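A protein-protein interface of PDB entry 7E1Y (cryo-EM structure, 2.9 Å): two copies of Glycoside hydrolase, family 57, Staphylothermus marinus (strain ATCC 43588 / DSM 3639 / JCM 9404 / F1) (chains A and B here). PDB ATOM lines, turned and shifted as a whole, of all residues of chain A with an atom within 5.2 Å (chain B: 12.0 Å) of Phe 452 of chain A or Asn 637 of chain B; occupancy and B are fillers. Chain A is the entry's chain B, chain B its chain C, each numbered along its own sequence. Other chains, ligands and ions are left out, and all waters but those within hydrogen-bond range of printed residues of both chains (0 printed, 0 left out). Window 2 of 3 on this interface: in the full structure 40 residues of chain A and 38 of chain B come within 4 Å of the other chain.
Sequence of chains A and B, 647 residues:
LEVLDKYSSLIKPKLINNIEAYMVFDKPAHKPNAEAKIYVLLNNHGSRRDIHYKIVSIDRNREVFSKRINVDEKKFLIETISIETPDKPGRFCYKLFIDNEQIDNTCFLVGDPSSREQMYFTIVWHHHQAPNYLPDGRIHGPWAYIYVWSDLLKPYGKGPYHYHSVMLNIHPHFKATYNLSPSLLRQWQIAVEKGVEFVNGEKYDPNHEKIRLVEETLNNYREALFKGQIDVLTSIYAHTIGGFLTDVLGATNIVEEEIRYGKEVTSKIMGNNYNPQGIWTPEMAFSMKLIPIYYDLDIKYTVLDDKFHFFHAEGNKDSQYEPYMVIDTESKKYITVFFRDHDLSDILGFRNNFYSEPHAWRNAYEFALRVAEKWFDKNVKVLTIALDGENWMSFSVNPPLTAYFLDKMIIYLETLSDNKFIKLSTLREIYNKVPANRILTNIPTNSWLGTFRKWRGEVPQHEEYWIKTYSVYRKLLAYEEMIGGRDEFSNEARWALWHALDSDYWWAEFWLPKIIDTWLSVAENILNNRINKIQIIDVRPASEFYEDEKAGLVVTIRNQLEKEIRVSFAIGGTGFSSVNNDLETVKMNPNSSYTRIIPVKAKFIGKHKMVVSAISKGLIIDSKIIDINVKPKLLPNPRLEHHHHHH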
ATOM      1  N   ILE A 241      -6.451  19.010 -11.054  1.00  0.00           N
ATOM      2  CA  ILE A 241      -6.661  20.248 -10.310  1.00  0.00           C
ATOM      3  C   ILE A 241      -6.680  21.426 -11.277  1.00  0.00           C
ATOM      4  O   ILE A 241      -5.633  21.952 -11.668  1.00  0.00           O
ATOM      5  CB  ILE A 241      -5.600  20.409  -9.204  1.00  0.00           C
ATOM      6  CG1 ILE A 241      -4.199  20.094  -9.731  1.00  0.00           C
ATOM      7  CG2 ILE A 241      -5.922  19.512  -8.029  1.00  0.00           C
ATOM      8  CD1 ILE A 241      -3.106  20.363  -8.732  1.00  0.00           C
ATOM      9  N   GLY A 243      -7.809  24.745 -11.256  1.00  0.00           N
ATOM     10  CA  GLY A 243      -7.305  26.063 -10.941  1.00  0.00           C
ATOM     11  C   GLY A 243      -5.807  26.159 -10.869  1.00  0.00           C
ATOM     12  O   GLY A 243      -5.241  27.193 -11.229  1.00  0.00           O
ATOM     13  N   PHE A 244      -5.149  25.101 -10.410  1.00  0.00           N
ATOM     14  CA  PHE A 244      -3.698  25.024 -10.425  1.00  0.00           C
ATOM     15  C   PHE A 244      -3.123  25.049 -11.830  1.00  0.00           C
ATOM     16  O   PHE A 244      -2.143  25.760 -12.074  1.00  0.00           O
ATOM     17  CB  PHE A 244      -3.248  23.745  -9.718  1.00  0.00           C
ATOM     18  CG  PHE A 244      -1.763  23.561  -9.667  1.00  0.00           C
ATOM     19  CD1 PHE A 244      -1.008  24.190  -8.698  1.00  0.00           C
ATOM     20  CD2 PHE A 244      -1.123  22.751 -10.587  1.00  0.00           C
ATOM     21  CE1 PHE A 244       0.352  24.011  -8.648  1.00  0.00           C
ATOM     22  CE2 PHE A 244       0.240  22.575 -10.542  1.00  0.00           C
ATOM     23  CZ  PHE A 244       0.978  23.205  -9.573  1.00  0.00           C
ATOM     24  N   VAL A 248      -0.753  28.121 -12.332  1.00  0.00           N
ATOM     25  CA  VAL A 248       0.671  27.816 -12.285  1.00  0.00           C
ATOM     26  C   VAL A 248       1.178  27.449 -13.673  1.00  0.00           C
ATOM     27  O   VAL A 248       2.048  28.129 -14.225  1.00  0.00           O
ATOM     28  CB  VAL A 248       0.962  26.694 -11.275  1.00  0.00           C
ATOM     29  CG1 VAL A 248       2.373  26.170 -11.455  1.00  0.00           C
ATOM     30  CG2 VAL A 248       0.760  27.204  -9.870  1.00  0.00           C
ATOM     31  N   ALA A 285     -10.699  22.814  -6.949  1.00  0.00           N
ATOM     32  CA  ALA A 285      -9.573  23.702  -7.217  1.00  0.00           C
ATOM     33  C   ALA A 285     -10.044  24.705  -8.263  1.00  0.00           C
ATOM     34  O   ALA A 285      -9.908  24.494  -9.467  1.00  0.00           O
ATOM     35  CB  ALA A 285      -8.355  22.921  -7.680  1.00  0.00           C
ATOM     36  N   THR A 445      -8.020  31.450  -5.883  1.00  0.00           N
ATOM     37  CA  THR A 445      -7.713  30.074  -6.250  1.00  0.00           C
ATOM     38  C   THR A 445      -7.386  29.247  -5.015  1.00  0.00           C
ATOM     39  O   THR A 445      -6.535  29.632  -4.209  1.00  0.00           O
ATOM     40  CB  THR A 445      -6.539  30.046  -7.225  1.00  0.00           C
ATOM     41  OG1 THR A 445      -6.834  30.876  -8.354  1.00  0.00           O
ATOM     42  CG2 THR A 445      -6.281  28.636  -7.711  1.00  0.00           C
ATOM     43  N   ASN A 446      -8.045  28.097  -4.881  1.00  0.00           N
ATOM     44  CA  ASN A 446      -7.903  27.267  -3.693  1.00  0.00           C
ATOM     45  C   ASN A 446      -8.661  25.966  -3.921  1.00  0.00           C
ATOM     46  O   ASN A 446      -9.539  25.891  -4.780  1.00  0.00           O
ATOM     47  CB  ASN A 446      -8.429  28.001  -2.454  1.00  0.00           C
ATOM     48  CG  ASN A 446      -7.700  27.616  -1.193  1.00  0.00           C
ATOM     49  OD1 ASN A 446      -6.914  26.675  -1.180  1.00  0.00           O
ATOM     50  ND2 ASN A 446      -7.940  28.363  -0.126  1.00  0.00           N
ATOM     51  N   SER A 447      -8.297  24.938  -3.153  1.00  0.00           N
ATOM     52  CA  SER A 447      -8.985  23.651  -3.096  1.00  0.00           C
ATOM     53  C   SER A 447      -9.701  23.535  -1.750  1.00  0.00           C
ATOM     54  O   SER A 447      -9.710  24.484  -0.962  1.00  0.00           O
ATOM     55  CB  SER A 447      -7.983  22.520  -3.328  1.00  0.00           C
ATOM     56  OG  SER A 447      -6.969  22.526  -2.345  1.00  0.00           O
ATOM     57  N   GLY A 450      -7.254  23.895   1.341  1.00  0.00           N
ATOM     58  CA  GLY A 450      -6.685  25.159   1.752  1.00  0.00           C
ATOM     59  C   GLY A 450      -5.298  25.413   1.224  1.00  0.00           C
ATOM     60  O   GLY A 450      -4.676  26.410   1.593  1.00  0.00           O
ATOM     61  N   THR A 451      -4.796  24.532   0.366  1.00  0.00           N
ATOM     62  CA  THR A 451      -3.454  24.659  -0.174  1.00  0.00           C
ATOM     63  C   THR A 451      -3.361  23.800  -1.422  1.00  0.00           C
ATOM     64  O   THR A 451      -4.207  22.939  -1.670  1.00  0.00           O
ATOM     65  CB  THR A 451      -2.394  24.241   0.850  1.00  0.00           C
ATOM     66  OG1 THR A 451      -1.103  24.685   0.415  1.00  0.00           O
ATOM     67  CG2 THR A 451      -2.379  22.730   1.011  1.00  0.00           C
ATOM     68  N   PHE A 452      -2.323  24.056  -2.212  1.00  0.00           N
ATOM     69  CA  PHE A 452      -1.997  23.221  -3.357  1.00  0.00           C
ATOM     70  C   PHE A 452      -0.747  22.392  -3.113  1.00  0.00           C
ATOM     71  O   PHE A 452      -0.238  21.765  -4.044  1.00  0.00           O
ATOM     72  CB  PHE A 452      -1.836  24.083  -4.607  1.00  0.00           C
ATOM     73  CG  PHE A 452      -3.134  24.435  -5.258  1.00  0.00           C
ATOM     74  CD1 PHE A 452      -3.946  23.449  -5.780  1.00  0.00           C
ATOM     75  CD2 PHE A 452      -3.553  25.747  -5.332  1.00  0.00           C
ATOM     76  CE1 PHE A 452      -5.141  23.767  -6.371  1.00  0.00           C
ATOM     77  CE2 PHE A 452      -4.747  26.066  -5.924  1.00  0.00           C
ATOM     78  CZ  PHE A 452      -5.541  25.078  -6.445  1.00  0.00           C
ATOM     79  N   ARG A 453      -0.258  22.362  -1.876  1.00  0.00           N
ATOM     80  CA  ARG A 453       0.973  21.670  -1.528  1.00  0.00           C
ATOM     81  C   ARG A 453       0.811  20.162  -1.470  1.00  0.00           C
ATOM     82  O   ARG A 453       1.812  19.456  -1.331  1.00  0.00           O
ATOM     83  CB  ARG A 453       1.487  22.178  -0.184  1.00  0.00           C
ATOM     84  CG  ARG A 453       2.413  23.366  -0.297  1.00  0.00           C
ATOM     85  CD  ARG A 453       3.102  23.637   1.021  1.00  0.00           C
ATOM     86  NE  ARG A 453       3.443  22.402   1.718  1.00  0.00           N
ATOM     87  CZ  ARG A 453       4.655  21.862   1.730  1.00  0.00           C
ATOM     88  NH1 ARG A 453       5.650  22.448   1.079  1.00  0.00           N
ATOM     89  NH2 ARG A 453       4.873  20.737   2.394  1.00  0.00           N
ATOM     90  N   LYS A 454      -0.413  19.653  -1.567  1.00  0.00           N
ATOM     91  CA  LYS A 454      -0.617  18.213  -1.576  1.00  0.00           C
ATOM     92  C   LYS A 454      -0.196  17.587  -2.898  1.00  0.00           C
ATOM     93  O   LYS A 454       0.239  16.431  -2.910  1.00  0.00           O
ATOM     94  CB  LYS A 454      -2.083  17.903  -1.265  1.00  0.00           C
ATOM     95  CG  LYS A 454      -2.500  16.472  -1.507  1.00  0.00           C
ATOM     96  CD  LYS A 454      -1.892  15.556  -0.467  1.00  0.00           C
ATOM     97  CE  LYS A 454      -2.589  15.685   0.869  1.00  0.00           C
ATOM     98  NZ  LYS A 454      -1.973  14.794   1.884  1.00  0.00           N
ATOM     99  N   TRP A 455      -0.289  18.327  -4.004  1.00  0.00           N
ATOM    100  CA  TRP A 455       0.181  17.851  -5.296  1.00  0.00           C
ATOM    101  C   TRP A 455       1.433  18.556  -5.783  1.00  0.00           C
ATOM    102  O   TRP A 455       1.935  18.207  -6.854  1.00  0.00           O
ATOM    103  CB  TRP A 455      -0.910  18.010  -6.362  1.00  0.00           C
ATOM    104  CG  TRP A 455      -2.247  17.572  -5.902  1.00  0.00           C
ATOM    105  CD1 TRP A 455      -2.804  16.344  -6.058  1.00  0.00           C
ATOM    106  CD2 TRP A 455      -3.210  18.366  -5.209  1.00  0.00           C
ATOM    107  NE1 TRP A 455      -4.055  16.318  -5.502  1.00  0.00           N
ATOM    108  CE2 TRP A 455      -4.327  17.551  -4.972  1.00  0.00           C
ATOM    109  CE3 TRP A 455      -3.234  19.688  -4.762  1.00  0.00           C
ATOM    110  CZ2 TRP A 455      -5.452  18.011  -4.306  1.00  0.00           C
ATOM    111  CZ3 TRP A 455      -4.352  20.142  -4.106  1.00  0.00           C
ATOM    112  CH2 TRP A 455      -5.446  19.309  -3.884  1.00  0.00           C
ATOM    113  N   ARG A 456       1.937  19.549  -5.045  1.00  0.00           N
ATOM    114  CA  ARG A 456       3.219  20.178  -5.356  1.00  0.00           C
ATOM    115  C   ARG A 456       3.848  20.672  -4.051  1.00  0.00           C
ATOM    116  O   ARG A 456       3.566  21.774  -3.580  1.00  0.00           O
ATOM    117  CB  ARG A 456       3.052  21.314  -6.358  1.00  0.00           C
ATOM    118  CG  ARG A 456       4.368  21.880  -6.830  1.00  0.00           C
ATOM    119  CD  ARG A 456       4.173  23.096  -7.689  1.00  0.00           C
ATOM    120  NE  ARG A 456       5.452  23.643  -8.118  1.00  0.00           N
ATOM    121  CZ  ARG A 456       5.592  24.802  -8.744  1.00  0.00           C
ATOM    122  NH1 ARG A 456       4.527  25.545  -9.003  1.00  0.00           N
ATOM    123  NH2 ARG A 456       6.795  25.224  -9.102  1.00  0.00           N
ATOM    124  N   LYS B 633      11.543  27.630 -16.394  1.00  0.00           N
ATOM    125  CA  LYS B 633      11.283  28.108 -15.043  1.00  0.00           C
ATOM    126  C   LYS B 633       9.795  28.009 -14.743  1.00  0.00           C
ATOM    127  O   LYS B 633       8.979  28.680 -15.384  1.00  0.00           O
ATOM    128  CB  LYS B 633      11.765  29.546 -14.886  1.00  0.00           C
ATOM    129  CG  LYS B 633      12.248  29.885 -13.488  1.00  0.00           C
ATOM    130  CD  LYS B 633      12.454  31.380 -13.332  1.00  0.00           C
ATOM    131  CE  LYS B 633      13.511  31.901 -14.288  1.00  0.00           C
ATOM    132  NZ  LYS B 633      14.273  33.040 -13.705  1.00  0.00           N
ATOM    133  N   LEU B 634       9.441  27.177 -13.773  1.00  0.00           N
ATOM    134  CA  LEU B 634       8.055  26.966 -13.390  1.00  0.00           C
ATOM    135  C   LEU B 634       7.663  27.927 -12.276  1.00  0.00           C
ATOM    136  O   LEU B 634       8.458  28.207 -11.374  1.00  0.00           O
ATOM    137  CB  LEU B 634       7.835  25.522 -12.939  1.00  0.00           C
ATOM    138  CG  LEU B 634       6.423  24.970 -13.114  1.00  0.00           C
ATOM    139  CD1 LEU B 634       5.868  25.390 -14.459  1.00  0.00           C
ATOM    140  CD2 LEU B 634       6.418  23.459 -12.973  1.00  0.00           C
ATOM    141  N   LEU B 635       6.435  28.430 -12.344  1.00  0.00           N
ATOM    142  CA  LEU B 635       5.927  29.367 -11.354  1.00  0.00           C
ATOM    143  C   LEU B 635       5.507  28.625 -10.091  1.00  0.00           C
ATOM    144  O   LEU B 635       5.083  27.470 -10.141  1.00  0.00           O
ATOM    145  CB  LEU B 635       4.756  30.152 -11.940  1.00  0.00           C
ATOM    146  CG  LEU B 635       5.107  31.449 -12.675  1.00  0.00           C
ATOM    147  CD1 LEU B 635       3.931  31.925 -13.516  1.00  0.00           C
ATOM    148  CD2 LEU B 635       5.541  32.528 -11.696  1.00  0.00           C
ATOM    149  N   PRO B 636       5.617  29.269  -8.931  1.00  0.00           N
ATOM    150  CA  PRO B 636       5.247  28.616  -7.673  1.00  0.00           C
ATOM    151  C   PRO B 636       3.738  28.524  -7.479  1.00  0.00           C
ATOM    152  O   PRO B 636       2.942  29.021  -8.277  1.00  0.00           O
ATOM    153  CB  PRO B 636       5.872  29.531  -6.605  1.00  0.00           C
ATOM    154  CG  PRO B 636       6.902  30.338  -7.338  1.00  0.00           C
ATOM    155  CD  PRO B 636       6.320  30.539  -8.698  1.00  0.00           C
ATOM    156  N   ASN B 637       3.362  27.871  -6.381  1.00  0.00           N
ATOM    157  CA  ASN B 637       1.958  27.708  -6.042  1.00  0.00           C
ATOM    158  C   ASN B 637       1.328  29.056  -5.702  1.00  0.00           C
ATOM    159  O   ASN B 637       2.019  29.981  -5.266  1.00  0.00           O
ATOM    160  CB  ASN B 637       1.797  26.775  -4.844  1.00  0.00           C
ATOM    161  CG  ASN B 637       2.151  25.355  -5.162  1.00  0.00           C
ATOM    162  OD1 ASN B 637       2.074  24.933  -6.308  1.00  0.00           O
ATOM    163  ND2 ASN B 637       2.536  24.600  -4.145  1.00  0.00           N
ATOM    164  N   PRO B 638       0.018  29.198  -5.898  1.00  0.00           N
ATOM    165  CA  PRO B 638      -0.697  30.296  -5.240  1.00  0.00           C
ATOM    166  C   PRO B 638      -0.531  30.181  -3.735  1.00  0.00           C
ATOM    167  O   PRO B 638      -0.671  29.085  -3.182  1.00  0.00           O
ATOM    168  CB  PRO B 638      -2.154  30.091  -5.671  1.00  0.00           C
ATOM    169  CG  PRO B 638      -2.087  29.279  -6.908  1.00  0.00           C
ATOM    170  CD  PRO B 638      -0.822  28.473  -6.866  1.00  0.00           C
ATOM    171  N   ARG B 639      -0.228  31.285  -3.058  1.00  0.00           N
ATOM    172  CA  ARG B 639       0.049  31.217  -1.629  1.00  0.00           C
ATOM    173  C   ARG B 639      -1.229  30.901  -0.866  1.00  0.00           C
ATOM    174  O   ARG B 639      -2.073  31.778  -0.661  1.00  0.00           O
ATOM    175  CB  ARG B 639       0.662  32.530  -1.146  1.00  0.00           C
ATOM    176  CG  ARG B 639       1.198  32.470   0.274  1.00  0.00           C
ATOM    177  CD  ARG B 639       1.875  33.773   0.663  1.00  0.00           C
ATOM    178  NE  ARG B 639       3.059  34.028  -0.154  1.00  0.00           N
ATOM    179  CZ  ARG B 639       4.264  33.522   0.093  1.00  0.00           C
ATOM    180  NH1 ARG B 639       4.451  32.726   1.136  1.00  0.00           N
ATOM    181  NH2 ARG B 639       5.282  33.809  -0.706  1.00  0.00           N
ATOM    182  N   LEU B 640      -1.355  29.644  -0.444  1.00  0.00           N
ATOM    183  CA  LEU B 640      -2.575  29.110   0.155  1.00  0.00           C
ATOM    184  C   LEU B 640      -3.763  29.285  -0.788  1.00  0.00           C
ATOM    185  O   LEU B 640      -4.394  30.341  -0.826  1.00  0.00           O
ATOM    186  CB  LEU B 640      -2.857  29.771   1.507  1.00  0.00           C
ATOM    187  CG  LEU B 640      -1.906  29.418   2.655  1.00  0.00           C
ATOM    188  CD1 LEU B 640      -2.241  30.220   3.898  1.00  0.00           C
ATOM    189  CD2 LEU B 640      -1.940  27.929   2.960  1.00  0.00           C
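O of Leu 635 of chain B is in hydrogen-bond range of NH2 of Arg 456 of chain A (3.0 Å). ND2 of Asn 637 of chain B lies within hydrogen-bond range of O of Arg 456 of chain A, 3.1 Å away.
OD1 of Asn 637 of chain B touches CE1 of Phe 244 of chain A, 3.0 Å away. Val 248 of chain A touches Leu 635 of chain B (CG1 to O, 3.3 Å). Val 248 of chain A touches Pro 636 of chain B. CD of Pro 638 of chain B touches CG2 of Val 248 of chain A (3.6 Å). Gly 450 of chain A touches Leu 640 of chain B. ND2 of Asn 637 of chain B touches O of Phe 452 of chain A, 3.97 Å away. Arg 456 of chain A touches Leu 634 of chain B (NH2 to CB, 3.99 Å). Pro 636 of chain B touches Arg 456 of chain A.
Of chain A, only Phe 244 (3.0 Å), Phe 452 (3.97 Å) and Arg 456 (3.1 Å) come within 4 Å of Asn 637 of chain B. No residue of chain B comes within 4 Å of Ile 241 of chain A. No residue of chain B comes within 4 Å of Gly 243 of chain A. No residue of chain B comes within 4 Å of Ala 285 of chain A. No residue of chain B comes within 4 Å of Thr 445 of chain A. No residue of chain B comes within 4 Å of Asn 446 of chain A. No residue of chain B comes within 4 Å of Ser 447 of chain A. Of the printed residues of chain B, Gly 450 of chain A touches Leu 640. No residue of chain B comes within 4 Å of Thr 451 of chain A. No residue of chain B comes within 4 Å of Arg 453 of chain A. No residue of chain B comes within 4 Å of Trp 455 of chain A. Printed residues of chain A within 4 Å of Leu 635 of chain B: Val 248 (3.3 Å) and Arg 456 (2.3 Å). Printed residues of chain B within 4 Å of Val 248 of chain A: Leu 635, Pro 636 and Pro 638. Of the printed residues of chain B, Arg 456 of chain A touches Leu 634 (3.99 Å), Leu 635 (2.3 Å), Pro 636 (3.4 Å) and Asn 637 (3.1 Å). Of the printed residues of chain A, Pro 638 of chain B touches Val 248 (3.6 Å). Of the printed residues of chain A, Pro 636 of chain B touches Val 248 and Arg 456. The nearest printed residue of chain A that does not touch Asn 637 of chain B is Val 248 of chain A (4.04 Å). The nearest printed residue of chain A that does not touch Leu 640 of chain B is Thr 445 of chain A (4.1 Å).
Of the 15 printed residues of chain A, 5 touch a printed residue of chain B. Printed residues of chain A that touch a printed residue of chain B: Phe 244, Val 248, Gly 450, Phe 452 and Arg 456. Hydrophobic or aromatic side chains of chain A within 4 Å of the printed part of chain B: Phe 244 and Val 248. Of the 8 printed residues of chain B, 6 touch a printed residue of chain A. Among the printed residues, 10 pairs touch across the chains. Among the printed residues, no Asp or Glu carboxylate lies within 4 Å of a Lys or Arg side-chain nitrogen of the other chain.
No position is printed for both chains. Of the 10 pairs that touch across the chains among the printed residues, none has its exchanged pair printed and touching as well.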
